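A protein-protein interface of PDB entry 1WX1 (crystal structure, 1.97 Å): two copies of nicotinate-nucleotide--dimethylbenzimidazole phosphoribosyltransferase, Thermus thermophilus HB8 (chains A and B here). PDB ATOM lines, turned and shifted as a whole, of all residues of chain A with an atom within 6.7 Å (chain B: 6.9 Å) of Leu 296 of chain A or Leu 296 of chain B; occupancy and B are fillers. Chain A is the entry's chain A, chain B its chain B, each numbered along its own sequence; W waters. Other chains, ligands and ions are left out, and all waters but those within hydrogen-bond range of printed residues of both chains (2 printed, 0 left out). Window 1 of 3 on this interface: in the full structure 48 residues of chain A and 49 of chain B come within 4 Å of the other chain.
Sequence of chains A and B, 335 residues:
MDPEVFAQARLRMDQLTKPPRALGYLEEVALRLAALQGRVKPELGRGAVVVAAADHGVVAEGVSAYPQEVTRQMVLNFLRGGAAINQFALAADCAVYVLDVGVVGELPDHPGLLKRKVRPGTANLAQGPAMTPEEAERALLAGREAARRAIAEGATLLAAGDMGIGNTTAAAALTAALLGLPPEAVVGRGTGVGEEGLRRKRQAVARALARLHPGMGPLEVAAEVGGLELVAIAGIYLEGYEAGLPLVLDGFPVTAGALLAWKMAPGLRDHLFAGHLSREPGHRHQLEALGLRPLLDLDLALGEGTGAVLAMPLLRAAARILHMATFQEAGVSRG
Arg 293 of chain A touches Asp 297 of chain B, and with the chains exchanged Asp 297 of chain A touches Arg 293 of chain B. Leu 295 of chain A touches Leu 298 of chain B, and with the chains exchanged Leu 298 of chain A touches Leu 295 of chain B. Leu 296 of chain B touches its own counterpart, Leu 296 of chain A. Of the 5 pairs that touch across the chains among the printed residues, 5 have their exchanged pair printed and touching as well.
Printed residues of chain B within 4 Å of Leu 295 of chain A: Leu 298. Of the printed residues of chain B, Asp 297 of chain A touches Arg 293 (3.3 Å). Leu 277 of chain B touches none of the printed residues of chain A. Printed residues of chain A within 4 Å of Leu 295 of chain B: Leu 298. Leu 296 of chain B touches one residue of chain A. Of the printed residues of chain A, Asp 297 of chain B touches Arg 293 (3.3 Å). Printed residues of chain A within 4 Å of Leu 298 of chain B: Leu 295 (3.5 Å). The nearest residue of chain B that does not touch Leu 296 of chain A is Leu 314 of chain B (4.1 Å).
The guanidinium group (NH2) of Arg 293 of chain A sits at hydrogen-bond distance from the backbone carbonyl oxygen (O) of Asp 297 of chain B (3.3 Å). O of Asp 297 of chain A sits at hydrogen-bond distance from NH2 of Arg 293 of chain B.
Water W1 lies within hydrogen-bond range of O of Leu 295 of chain A and N of Asp 297 of chain B. Water W2 lies within hydrogen-bond range of the backbone carbonyl oxygen of Leu 295 of chain B (2.7 Å) and the backbone NH of Asp 297 of chain A (2.9 Å).
Of the 21 printed residues of chain B, 5 touch a printed residue of chain A. Among the printed residues, 5 pairs touch across the chains. Among the printed residues, no Asp or Glu carboxylate lies within 4 Å of a Lys or Arg side-chain nitrogen of the other chain.
Among the printed residues, pairs that only touch across the chains: Leu 295 of chain A with Leu 298 of chain B (3.5 Å), Leu 296 of chain A with Leu 296 of chain B (3.3 Å) and Leu 298 of chain A with Leu 295 of chain B (3.5 Å).
The backbone carbonyl oxygen (O) of Ala 274 of chain A is in hydrogen-bond range of the backbone NH (N) of Leu 295 of chain A (3.0 Å). O of Gly 275 of chain A is in hydrogen-bond range of N of Leu 296 of chain A, 3.0 Å away. The backbone carbonyl oxygen (O) of Ala 274 of chain B lies within hydrogen-bond range of the backbone NH (N) of Leu 295 of chain B, at 3.0 Å. N of Leu 296 of chain B sits at hydrogen-bond distance from O of Gly 275 of chain B (3.0 Å). The backbone NH of Leu 277 of chain B sits at hydrogen-bond distance from the backbone carbonyl oxygen of Leu 296 of chain B, at 2.9 Å.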
ATOM      1  N   ALA A 274      21.965 -12.904 -14.660  1.00  0.00           N
ATOM      2  CA  ALA A 274      21.937 -13.635 -15.920  1.00  0.00           C
ATOM      3  C   ALA A 274      20.566 -13.485 -16.565  1.00  0.00           C
ATOM      4  O   ALA A 274      19.573 -14.039 -16.080  1.00  0.00           O
ATOM      5  CB  ALA A 274      22.261 -15.111 -15.688  1.00  0.00           C
ATOM      6  N   GLY A 275      20.517 -12.727 -17.658  1.00  0.00           N
ATOM      7  CA  GLY A 275      19.261 -12.506 -18.354  1.00  0.00           C
ATOM      8  C   GLY A 275      18.602 -13.778 -18.856  1.00  0.00           C
ATOM      9  O   GLY A 275      17.410 -13.995 -18.640  1.00  0.00           O
ATOM     10  N   HIS A 276      19.368 -14.627 -19.532  1.00  0.00           N
ATOM     11  CA  HIS A 276      18.813 -15.871 -20.051  1.00  0.00           C
ATOM     12  C   HIS A 276      19.884 -16.927 -20.248  1.00  0.00           C
ATOM     13  O   HIS A 276      21.062 -16.707 -19.963  1.00  0.00           O
ATOM     14  CB  HIS A 276      18.115 -15.631 -21.393  1.00  0.00           C
ATOM     15  CG  HIS A 276      19.059 -15.387 -22.530  1.00  0.00           C
ATOM     16  ND1 HIS A 276      18.898 -15.970 -23.765  1.00  0.00           N
ATOM     17  CD2 HIS A 276      20.173 -14.618 -22.615  1.00  0.00           C
ATOM     18  CE1 HIS A 276      19.875 -15.575 -24.568  1.00  0.00           C
ATOM     19  NE2 HIS A 276      20.659 -14.755 -23.893  1.00  0.00           N
ATOM     20  N   LEU A 277      19.454 -18.085 -20.733  1.00  0.00           N
ATOM     21  CA  LEU A 277      20.364 -19.184 -21.020  1.00  0.00           C
ATOM     22  C   LEU A 277      20.312 -19.388 -22.527  1.00  0.00           C
ATOM     23  O   LEU A 277      19.276 -19.770 -23.076  1.00  0.00           O
ATOM     24  CB  LEU A 277      19.927 -20.469 -20.306  1.00  0.00           C
ATOM     25  CG  LEU A 277      20.825 -21.683 -20.594  1.00  0.00           C
ATOM     26  CD1 LEU A 277      22.251 -21.399 -20.136  1.00  0.00           C
ATOM     27  CD2 LEU A 277      20.271 -22.916 -19.894  1.00  0.00           C
ATOM     28  N   SER A 278      21.428 -19.106 -23.189  1.00  0.00           N
ATOM     29  CA  SER A 278      21.534 -19.252 -24.632  1.00  0.00           C
ATOM     30  C   SER A 278      21.579 -20.725 -25.005  1.00  0.00           C
ATOM     31  O   SER A 278      21.854 -21.571 -24.160  1.00  0.00           O
ATOM     32  CB  SER A 278      22.810 -18.569 -25.136  1.00  0.00           C
ATOM     33  OG  SER A 278      23.023 -18.838 -26.509  1.00  0.00           O
ATOM     34  N   ARG A 293      22.013 -17.934 -11.877  1.00  0.00           N
ATOM     35  CA  ARG A 293      20.866 -18.657 -12.408  1.00  0.00           C
ATOM     36  C   ARG A 293      20.193 -17.793 -13.470  1.00  0.00           C
ATOM     37  O   ARG A 293      19.855 -16.640 -13.216  1.00  0.00           O
ATOM     38  CB  ARG A 293      19.856 -18.960 -11.299  1.00  0.00           C
ATOM     39  CG  ARG A 293      18.591 -19.654 -11.781  1.00  0.00           C
ATOM     40  CD  ARG A 293      17.599 -19.812 -10.638  1.00  0.00           C
ATOM     41  NE  ARG A 293      16.396 -20.548 -11.020  1.00  0.00           N
ATOM     42  CZ  ARG A 293      15.554 -20.178 -11.980  1.00  0.00           C
ATOM     43  NH1 ARG A 293      15.773 -19.069 -12.675  1.00  0.00           N
ATOM     44  NH2 ARG A 293      14.482 -20.917 -12.239  1.00  0.00           N
ATOM     45  N   PRO A 294      19.993 -18.344 -14.674  1.00  0.00           N
ATOM     46  CA  PRO A 294      19.356 -17.631 -15.789  1.00  0.00           C
ATOM     47  C   PRO A 294      17.885 -17.334 -15.490  1.00  0.00           C
ATOM     48  O   PRO A 294      17.148 -18.207 -15.030  1.00  0.00           O
ATOM     49  CB  PRO A 294      19.503 -18.601 -16.963  1.00  0.00           C
ATOM     50  CG  PRO A 294      20.623 -19.523 -16.545  1.00  0.00           C
ATOM     51  CD  PRO A 294      20.405 -19.698 -15.079  1.00  0.00           C
ATOM     52  N   LEU A 295      17.457 -16.107 -15.760  1.00  0.00           N
ATOM     53  CA  LEU A 295      16.070 -15.725 -15.518  1.00  0.00           C
ATOM     54  C   LEU A 295      15.134 -16.286 -16.580  1.00  0.00           C
ATOM     55  O   LEU A 295      14.025 -16.717 -16.274  1.00  0.00           O
ATOM     56  CB  LEU A 295      15.937 -14.203 -15.492  1.00  0.00           C
ATOM     57  CG  LEU A 295      16.468 -13.520 -14.238  1.00  0.00           C
ATOM     58  CD1 LEU A 295      16.460 -12.012 -14.425  1.00  0.00           C
ATOM     59  CD2 LEU A 295      15.606 -13.920 -13.055  1.00  0.00           C
ATOM     60  N   LEU A 296      15.588 -16.265 -17.829  1.00  0.00           N
ATOM     61  CA  LEU A 296      14.797 -16.756 -18.950  1.00  0.00           C
ATOM     62  C   LEU A 296      15.473 -17.923 -19.659  1.00  0.00           C
ATOM     63  O   LEU A 296      16.697 -18.043 -19.655  1.00  0.00           O
ATOM     64  CB  LEU A 296      14.593 -15.638 -19.977  1.00  0.00           C
ATOM     65  CG  LEU A 296      13.862 -14.374 -19.526  1.00  0.00           C
ATOM     66  CD1 LEU A 296      14.025 -13.280 -20.581  1.00  0.00           C
ATOM     67  CD2 LEU A 296      12.396 -14.697 -19.296  1.00  0.00           C
ATOM     68  N   ASP A 297      14.660 -18.773 -20.275  1.00  0.00           N
ATOM     69  CA  ASP A 297      15.157 -19.904 -21.050  1.00  0.00           C
ATOM     70  C   ASP A 297      14.183 -20.050 -22.212  1.00  0.00           C
ATOM     71  O   ASP A 297      13.206 -20.795 -22.126  1.00  0.00           O
ATOM     72  CB  ASP A 297      15.175 -21.188 -20.230  1.00  0.00           C
ATOM     73  CG  ASP A 297      15.940 -22.299 -20.925  1.00  0.00           C
ATOM     74  OD1 ASP A 297      16.028 -22.264 -22.170  1.00  0.00           O
ATOM     75  OD2 ASP A 297      16.447 -23.208 -20.235  1.00  0.00           O
ATOM     76  N   LEU A 298      14.449 -19.324 -23.293  1.00  0.00           N
ATOM     77  CA  LEU A 298      13.574 -19.342 -24.455  1.00  0.00           C
ATOM     78  C   LEU A 298      14.238 -19.925 -25.697  1.00  0.00           C
ATOM     79  O   LEU A 298      13.755 -19.732 -26.809  1.00  0.00           O
ATOM     80  CB  LEU A 298      13.088 -17.919 -24.742  1.00  0.00           C
ATOM     81  CG  LEU A 298      12.300 -17.246 -23.612  1.00  0.00           C
ATOM     82  CD1 LEU A 298      12.177 -15.753 -23.889  1.00  0.00           C
ATOM     83  CD2 LEU A 298      10.926 -17.893 -23.480  1.00  0.00           C
ATOM     84  N   ASP A 299      15.344 -20.635 -25.493  1.00  0.00           N
ATOM     85  CA  ASP A 299      16.086 -21.257 -26.583  1.00  0.00           C
ATOM     86  C   ASP A 299      16.571 -20.227 -27.601  1.00  0.00           C
ATOM     87  O   ASP A 299      16.604 -20.489 -28.806  1.00  0.00           O
ATOM     88  CB  ASP A 299      15.218 -22.324 -27.265  1.00  0.00           C
ATOM     89  CG  ASP A 299      15.977 -23.112 -28.321  1.00  0.00           C
ATOM     90  OD1 ASP A 299      17.153 -23.458 -28.083  1.00  0.00           O
ATOM     91  OD2 ASP A 299      15.390 -23.395 -29.389  1.00  0.00           O
ATOM     92  N   LEU A 300      16.952 -19.054 -27.107  1.00  0.00           N
ATOM     93  CA  LEU A 300      17.447 -17.989 -27.967  1.00  0.00           C
ATOM     94  C   LEU A 300      18.899 -18.271 -28.340  1.00  0.00           C
ATOM     95  O   LEU A 300      19.656 -18.835 -27.553  1.00  0.00           O
ATOM     96  CB  LEU A 300      17.357 -16.639 -27.248  1.00  0.00           C
ATOM     97  CG  LEU A 300      15.976 -16.232 -26.724  1.00  0.00           C
ATOM     98  CD1 LEU A 300      16.085 -14.902 -25.994  1.00  0.00           C
ATOM     99  CD2 LEU A 300      14.988 -16.131 -27.875  1.00  0.00           C
ATOM    100  N   THR A 306      19.878  -9.256 -26.806  1.00  0.00           N
ATOM    101  CA  THR A 306      18.452  -9.574 -26.791  1.00  0.00           C
ATOM    102  C   THR A 306      17.945 -10.239 -25.522  1.00  0.00           C
ATOM    103  O   THR A 306      16.922  -9.822 -24.974  1.00  0.00           O
ATOM    104  CB  THR A 306      18.055 -10.477 -27.981  1.00  0.00           C
ATOM    105  OG1 THR A 306      18.900 -11.631 -28.010  1.00  0.00           O
ATOM    106  CG2 THR A 306      18.177  -9.718 -29.299  1.00  0.00           C
ATOM    107  N   GLY A 307      18.643 -11.275 -25.065  1.00  0.00           N
ATOM    108  CA  GLY A 307      18.215 -11.973 -23.866  1.00  0.00           C
ATOM    109  C   GLY A 307      18.259 -11.085 -22.640  1.00  0.00           C
ATOM    110  O   GLY A 307      17.362 -11.130 -21.797  1.00  0.00           O
ATOM    111  N   ALA A 308      19.306 -10.272 -22.538  1.00  0.00           N
ATOM    112  CA  ALA A 308      19.455  -9.368 -21.414  1.00  0.00           C
ATOM    113  C   ALA A 308      18.321  -8.350 -21.371  1.00  0.00           C
ATOM    114  O   ALA A 308      17.769  -8.070 -20.306  1.00  0.00           O
ATOM    115  CB  ALA A 308      20.796  -8.644 -21.501  1.00  0.00           C
ATOM    116  N   VAL A 309      17.985  -7.790 -22.530  1.00  0.00           N
ATOM    117  CA  VAL A 309      16.927  -6.790 -22.616  1.00  0.00           C
ATOM    118  C   VAL A 309      15.555  -7.379 -22.291  1.00  0.00           C
ATOM    119  O   VAL A 309      14.732  -6.731 -21.635  1.00  0.00           O
ATOM    120  CB  VAL A 309      16.916  -6.127 -24.013  1.00  0.00           C
ATOM    121  CG1 VAL A 309      15.681  -5.243 -24.177  1.00  0.00           C
ATOM    122  CG2 VAL A 309      18.180  -5.283 -24.179  1.00  0.00           C
ATOM    123  N   LEU A 310      15.312  -8.608 -22.738  1.00  0.00           N
ATOM    124  CA  LEU A 310      14.044  -9.277 -22.457  1.00  0.00           C
ATOM    125  C   LEU A 310      13.878  -9.513 -20.958  1.00  0.00           C
ATOM    126  O   LEU A 310      12.760  -9.615 -20.456  1.00  0.00           O
ATOM    127  CB  LEU A 310      13.978 -10.619 -23.187  1.00  0.00           C
ATOM    128  CG  LEU A 310      13.799 -10.563 -24.707  1.00  0.00           C
ATOM    129  CD1 LEU A 310      13.874 -11.965 -25.286  1.00  0.00           C
ATOM    130  CD2 LEU A 310      12.459  -9.916 -25.034  1.00  0.00           C
ATOM    131  N   ALA A 311      14.995  -9.598 -20.240  1.00  0.00           N
ATOM    132  CA  ALA A 311      14.950  -9.834 -18.797  1.00  0.00           C
ATOM    133  C   ALA A 311      14.777  -8.574 -17.952  1.00  0.00           C
ATOM    134  O   ALA A 311      14.495  -8.661 -16.754  1.00  0.00           O
ATOM    135  CB  ALA A 311      16.206 -10.567 -18.356  1.00  0.00           C
ATOM    136  N   MET A 312      14.932  -7.401 -18.558  1.00  0.00           N
ATOM    137  CA  MET A 312      14.812  -6.167 -17.788  1.00  0.00           C
ATOM    138  C   MET A 312      13.454  -5.982 -17.118  1.00  0.00           C
ATOM    139  O   MET A 312      13.390  -5.564 -15.963  1.00  0.00           O
ATOM    140  CB  MET A 312      15.157  -4.955 -18.657  1.00  0.00           C
ATOM    141  CG  MET A 312      16.627  -4.924 -19.059  1.00  0.00           C
ATOM    142  SD  MET A 312      17.105  -3.403 -19.919  1.00  0.00           S
ATOM    143  CE  MET A 312      18.888  -3.578 -19.956  1.00  0.00           C
ATOM    144  N   LEU A 314      11.585  -8.168 -15.981  1.00  0.00           N
ATOM    145  CA  LEU A 314      11.556  -9.080 -14.840  1.00  0.00           C
ATOM    146  C   LEU A 314      12.323  -8.465 -13.679  1.00  0.00           C
ATOM    147  O   LEU A 314      11.913  -8.585 -12.525  1.00  0.00           O
ATOM    148  CB  LEU A 314      12.173 -10.433 -15.198  1.00  0.00           C
ATOM    149  CG  LEU A 314      11.398 -11.298 -16.187  1.00  0.00           C
ATOM    150  CD1 LEU A 314      12.139 -12.620 -16.377  1.00  0.00           C
ATOM    151  CD2 LEU A 314       9.990 -11.552 -15.655  1.00  0.00           C
ATOM    152  N   ALA B 274       0.555 -19.474 -22.217  1.00  0.00           N
ATOM    153  CA  ALA B 274       0.904 -19.811 -20.843  1.00  0.00           C
ATOM    154  C   ALA B 274       1.975 -18.857 -20.328  1.00  0.00           C
ATOM    155  O   ALA B 274       3.126 -18.894 -20.779  1.00  0.00           O
ATOM    156  CB  ALA B 274       1.399 -21.249 -20.762  1.00  0.00           C
ATOM    157  N   GLY B 275       1.591 -18.010 -19.378  1.00  0.00           N
ATOM    158  CA  GLY B 275       2.524 -17.050 -18.821  1.00  0.00           C
ATOM    159  C   GLY B 275       3.705 -17.687 -18.114  1.00  0.00           C
ATOM    160  O   GLY B 275       4.849 -17.277 -18.311  1.00  0.00           O
ATOM    161  N   HIS B 276       3.439 -18.689 -17.282  1.00  0.00           N
ATOM    162  CA  HIS B 276       4.521 -19.343 -16.566  1.00  0.00           C
ATOM    163  C   HIS B 276       4.177 -20.756 -16.128  1.00  0.00           C
ATOM    164  O   HIS B 276       3.064 -21.237 -16.333  1.00  0.00           O
ATOM    165  CB  HIS B 276       4.901 -18.531 -15.324  1.00  0.00           C
ATOM    166  CG  HIS B 276       3.893 -18.610 -14.220  1.00  0.00           C
ATOM    167  ND1 HIS B 276       4.254 -18.767 -12.895  1.00  0.00           N
ATOM    168  CD2 HIS B 276       2.542 -18.544 -14.234  1.00  0.00           C
ATOM    169  CE1 HIS B 276       3.167 -18.794 -12.147  1.00  0.00           C
ATOM    170  NE2 HIS B 276       2.112 -18.660 -12.932  1.00  0.00           N
ATOM    171  N   LEU B 277       5.161 -21.413 -15.530  1.00  0.00           N
ATOM    172  CA  LEU B 277       4.986 -22.758 -15.011  1.00  0.00           C
ATOM    173  C   LEU B 277       5.017 -22.629 -13.497  1.00  0.00           C
ATOM    174  O   LEU B 277       6.070 -22.372 -12.911  1.00  0.00           O
ATOM    175  CB  LEU B 277       6.123 -23.680 -15.457  1.00  0.00           C
ATOM    176  CG  LEU B 277       6.047 -25.071 -14.817  1.00  0.00           C
ATOM    177  CD1 LEU B 277       4.777 -25.762 -15.283  1.00  0.00           C
ATOM    178  CD2 LEU B 277       7.273 -25.899 -15.182  1.00  0.00           C
ATOM    179  N   SER B 278       3.856 -22.787 -12.870  1.00  0.00           N
ATOM    180  CA  SER B 278       3.756 -22.693 -11.421  1.00  0.00           C
ATOM    181  C   SER B 278       4.412 -23.894 -10.756  1.00  0.00           C
ATOM    182  O   SER B 278       4.564 -24.945 -11.372  1.00  0.00           O
ATOM    183  CB  SER B 278       2.293 -22.625 -10.991  1.00  0.00           C
ATOM    184  OG  SER B 278       2.190 -22.760  -9.585  1.00  0.00           O
ATOM    185  N   ARG B 293       3.373 -24.161 -24.072  1.00  0.00           N
ATOM    186  CA  ARG B 293       4.686 -24.116 -23.437  1.00  0.00           C
ATOM    187  C   ARG B 293       4.760 -22.830 -22.607  1.00  0.00           C
ATOM    188  O   ARG B 293       4.522 -21.740 -23.123  1.00  0.00           O
ATOM    189  CB  ARG B 293       5.786 -24.111 -24.502  1.00  0.00           C
ATOM    190  CG  ARG B 293       7.187 -23.883 -23.962  1.00  0.00           C
ATOM    191  CD  ARG B 293       8.185 -23.755 -25.106  1.00  0.00           C
ATOM    192  NE  ARG B 293       9.468 -23.211 -24.667  1.00  0.00           N
ATOM    193  CZ  ARG B 293      10.339 -23.860 -23.900  1.00  0.00           C
ATOM    194  NH1 ARG B 293      10.069 -25.088 -23.480  1.00  0.00           N
ATOM    195  NH2 ARG B 293      11.482 -23.279 -23.557  1.00  0.00           N
ATOM    196  N   PRO B 294       5.086 -22.946 -21.311  1.00  0.00           N
ATOM    197  CA  PRO B 294       5.183 -21.772 -20.435  1.00  0.00           C
ATOM    198  C   PRO B 294       6.304 -20.829 -20.862  1.00  0.00           C
ATOM    199  O   PRO B 294       7.409 -21.269 -21.176  1.00  0.00           O
ATOM    200  CB  PRO B 294       5.441 -22.388 -19.064  1.00  0.00           C
ATOM    201  CG  PRO B 294       6.228 -23.622 -19.408  1.00  0.00           C
ATOM    202  CD  PRO B 294       5.448 -24.171 -20.579  1.00  0.00           C
ATOM    203  N   LEU B 295       6.014 -19.535 -20.875  1.00  0.00           N
ATOM    204  CA  LEU B 295       7.001 -18.538 -21.259  1.00  0.00           C
ATOM    205  C   LEU B 295       8.036 -18.349 -20.161  1.00  0.00           C
ATOM    206  O   LEU B 295       9.219 -18.146 -20.434  1.00  0.00           O
ATOM    207  CB  LEU B 295       6.314 -17.203 -21.554  1.00  0.00           C
ATOM    208  CG  LEU B 295       5.579 -17.089 -22.891  1.00  0.00           C
ATOM    209  CD1 LEU B 295       4.732 -15.823 -22.919  1.00  0.00           C
ATOM    210  CD2 LEU B 295       6.597 -17.074 -24.018  1.00  0.00           C
ATOM    211  N   LEU B 296       7.583 -18.417 -18.916  1.00  0.00           N
ATOM    212  CA  LEU B 296       8.467 -18.241 -17.772  1.00  0.00           C
ATOM    213  C   LEU B 296       8.455 -19.458 -16.863  1.00  0.00           C
ATOM    214  O   LEU B 296       7.485 -20.208 -16.823  1.00  0.00           O
ATOM    215  CB  LEU B 296       8.029 -17.025 -16.953  1.00  0.00           C
ATOM    216  CG  LEU B 296       7.980 -15.662 -17.642  1.00  0.00           C
ATOM    217  CD1 LEU B 296       7.266 -14.654 -16.741  1.00  0.00           C
ATOM    218  CD2 LEU B 296       9.397 -15.210 -17.951  1.00  0.00           C
ATOM    219  N   ASP B 297       9.548 -19.640 -16.134  1.00  0.00           N
ATOM    220  CA  ASP B 297       9.676 -20.732 -15.178  1.00  0.00           C
ATOM    221  C   ASP B 297      10.519 -20.156 -14.050  1.00  0.00           C
ATOM    222  O   ASP B 297      11.740 -20.325 -14.015  1.00  0.00           O
ATOM    223  CB  ASP B 297      10.388 -21.930 -15.802  1.00  0.00           C
ATOM    224  CG  ASP B 297      10.305 -23.167 -14.932  1.00  0.00           C
ATOM    225  OD1 ASP B 297      10.060 -23.025 -13.713  1.00  0.00           O
ATOM    226  OD2 ASP B 297      10.497 -24.280 -15.462  1.00  0.00           O
ATOM    227  N   LEU B 298       9.856 -19.474 -13.125  1.00  0.00           N
ATOM    228  CA  LEU B 298      10.544 -18.829 -12.019  1.00  0.00           C
ATOM    229  C   LEU B 298      10.219 -19.423 -10.656  1.00  0.00           C
ATOM    230  O   LEU B 298      10.502 -18.816  -9.624  1.00  0.00           O
ATOM    231  CB  LEU B 298      10.208 -17.336 -12.038  1.00  0.00           C
ATOM    232  CG  LEU B 298      10.630 -16.631 -13.335  1.00  0.00           C
ATOM    233  CD1 LEU B 298       9.971 -15.259 -13.428  1.00  0.00           C
ATOM    234  CD2 LEU B 298      12.154 -16.515 -13.375  1.00  0.00           C
ATOM    235  N   ASP B 299       9.630 -20.614 -10.660  1.00  0.00           N
ATOM    236  CA  ASP B 299       9.266 -21.292  -9.425  1.00  0.00           C
ATOM    237  C   ASP B 299       8.269 -20.469  -8.615  1.00  0.00           C
ATOM    238  O   ASP B 299       8.332 -20.430  -7.385  1.00  0.00           O
ATOM    239  CB  ASP B 299      10.521 -21.574  -8.590  1.00  0.00           C
ATOM    240  CG  ASP B 299      10.230 -22.422  -7.368  1.00  0.00           C
ATOM    241  OD1 ASP B 299       9.369 -23.324  -7.463  1.00  0.00           O
ATOM    242  OD2 ASP B 299      10.867 -22.195  -6.316  1.00  0.00           O
ATOM    243  N   LEU B 300       7.345 -19.815  -9.315  1.00  0.00           N
ATOM    244  CA  LEU B 300       6.324 -19.004  -8.663  1.00  0.00           C
ATOM    245  C   LEU B 300       5.186 -19.899  -8.183  1.00  0.00           C
ATOM    246  O   LEU B 300       4.882 -20.914  -8.806  1.00  0.00           O
ATOM    247  CB  LEU B 300       5.760 -17.958  -9.632  1.00  0.00           C
ATOM    248  CG  LEU B 300       6.746 -16.997 -10.311  1.00  0.00           C
ATOM    249  CD1 LEU B 300       5.963 -15.973 -11.116  1.00  0.00           C
ATOM    250  CD2 LEU B 300       7.611 -16.303  -9.274  1.00  0.00           C
ATOM    251  N   THR B 306      -0.297 -13.101 -11.101  1.00  0.00           N
ATOM    252  CA  THR B 306       1.075 -12.598 -11.143  1.00  0.00           C
ATOM    253  C   THR B 306       1.949 -13.145 -12.271  1.00  0.00           C
ATOM    254  O   THR B 306       2.652 -12.385 -12.930  1.00  0.00           O
ATOM    255  CB  THR B 306       1.794 -12.849  -9.804  1.00  0.00           C
ATOM    256  OG1 THR B 306       1.681 -14.231  -9.450  1.00  0.00           O
ATOM    257  CG2 THR B 306       1.179 -11.994  -8.708  1.00  0.00           C
ATOM    258  N   GLY B 307       1.913 -14.457 -12.484  1.00  0.00           N
ATOM    259  CA  GLY B 307       2.723 -15.051 -13.535  1.00  0.00           C
ATOM    260  C   GLY B 307       2.275 -14.632 -14.921  1.00  0.00           C
ATOM    261  O   GLY B 307       3.083 -14.530 -15.848  1.00  0.00           O
ATOM    262  N   ALA B 308       0.978 -14.396 -15.067  1.00  0.00           N
ATOM    263  CA  ALA B 308       0.422 -13.977 -16.343  1.00  0.00           C
ATOM    264  C   ALA B 308       0.871 -12.556 -16.656  1.00  0.00           C
ATOM    265  O   ALA B 308       1.275 -12.256 -17.780  1.00  0.00           O
ATOM    266  CB  ALA B 308      -1.100 -14.042 -16.296  1.00  0.00           C
ATOM    267  N   VAL B 309       0.793 -11.684 -15.656  1.00  0.00           N
ATOM    268  CA  VAL B 309       1.179 -10.290 -15.826  1.00  0.00           C
ATOM    269  C   VAL B 309       2.674 -10.164 -16.087  1.00  0.00           C
ATOM    270  O   VAL B 309       3.100  -9.338 -16.899  1.00  0.00           O
ATOM    271  CB  VAL B 309       0.787  -9.453 -14.587  1.00  0.00           C
ATOM    272  CG1 VAL B 309       1.326  -8.037 -14.719  1.00  0.00           C
ATOM    273  CG2 VAL B 309      -0.738  -9.415 -14.459  1.00  0.00           C
ATOM    274  N   LEU B 310       3.468 -10.988 -15.408  1.00  0.00           N
ATOM    275  CA  LEU B 310       4.917 -10.973 -15.598  1.00  0.00           C
ATOM    276  C   LEU B 310       5.302 -11.314 -17.030  1.00  0.00           C
ATOM    277  O   LEU B 310       6.343 -10.882 -17.518  1.00  0.00           O
ATOM    278  CB  LEU B 310       5.595 -11.987 -14.674  1.00  0.00           C
ATOM    279  CG  LEU B 310       5.738 -11.628 -13.201  1.00  0.00           C
ATOM    280  CD1 LEU B 310       6.422 -12.778 -12.470  1.00  0.00           C
ATOM    281  CD2 LEU B 310       6.552 -10.346 -13.069  1.00  0.00           C
ATOM    282  N   ALA B 311       4.464 -12.097 -17.699  1.00  0.00           N
ATOM    283  CA  ALA B 311       4.751 -12.523 -19.062  1.00  0.00           C
ATOM    284  C   ALA B 311       4.313 -11.549 -20.143  1.00  0.00           C
ATOM    285  O   ALA B 311       4.713 -11.687 -21.302  1.00  0.00           O
ATOM    286  CB  ALA B 311       4.117 -13.897 -19.317  1.00  0.00           C
ATOM    287  N   MET B 312       3.503 -10.558 -19.782  1.00  0.00           N
ATOM    288  CA  MET B 312       3.022  -9.615 -20.784  1.00  0.00           C
ATOM    289  C   MET B 312       4.115  -8.895 -21.565  1.00  0.00           C
ATOM    290  O   MET B 312       3.996  -8.732 -22.775  1.00  0.00           O
ATOM    291  CB  MET B 312       2.054  -8.619 -20.152  1.00  0.00           C
ATOM    292  CG  MET B 312       0.780  -9.302 -19.652  1.00  0.00           C
ATOM    293  SD  MET B 312      -0.479  -8.154 -19.079  1.00  0.00           S
ATOM    294  CE  MET B 312      -1.865  -9.298 -18.767  1.00  0.00           C
ATOM    295  N   LEU B 314       6.989  -9.968 -22.365  1.00  0.00           N
ATOM    296  CA  LEU B 314       7.550 -10.938 -23.306  1.00  0.00           C
ATOM    297  C   LEU B 314       6.649 -11.100 -24.524  1.00  0.00           C
ATOM    298  O   LEU B 314       7.124 -11.255 -25.648  1.00  0.00           O
ATOM    299  CB  LEU B 314       7.727 -12.306 -22.640  1.00  0.00           C
ATOM    300  CG  LEU B 314       8.931 -12.526 -21.723  1.00  0.00           C
ATOM    301  CD1 LEU B 314       8.840 -13.908 -21.087  1.00  0.00           C
ATOM    302  CD2 LEU B 314      10.216 -12.390 -22.532  1.00  0.00           C
HETATM  303  O   HOH W   1      11.988 -18.435 -16.805  1.00  0.00           O
HETATM  304  O   HOH W   2      11.805 -18.774 -19.787  1.00  0.00           O
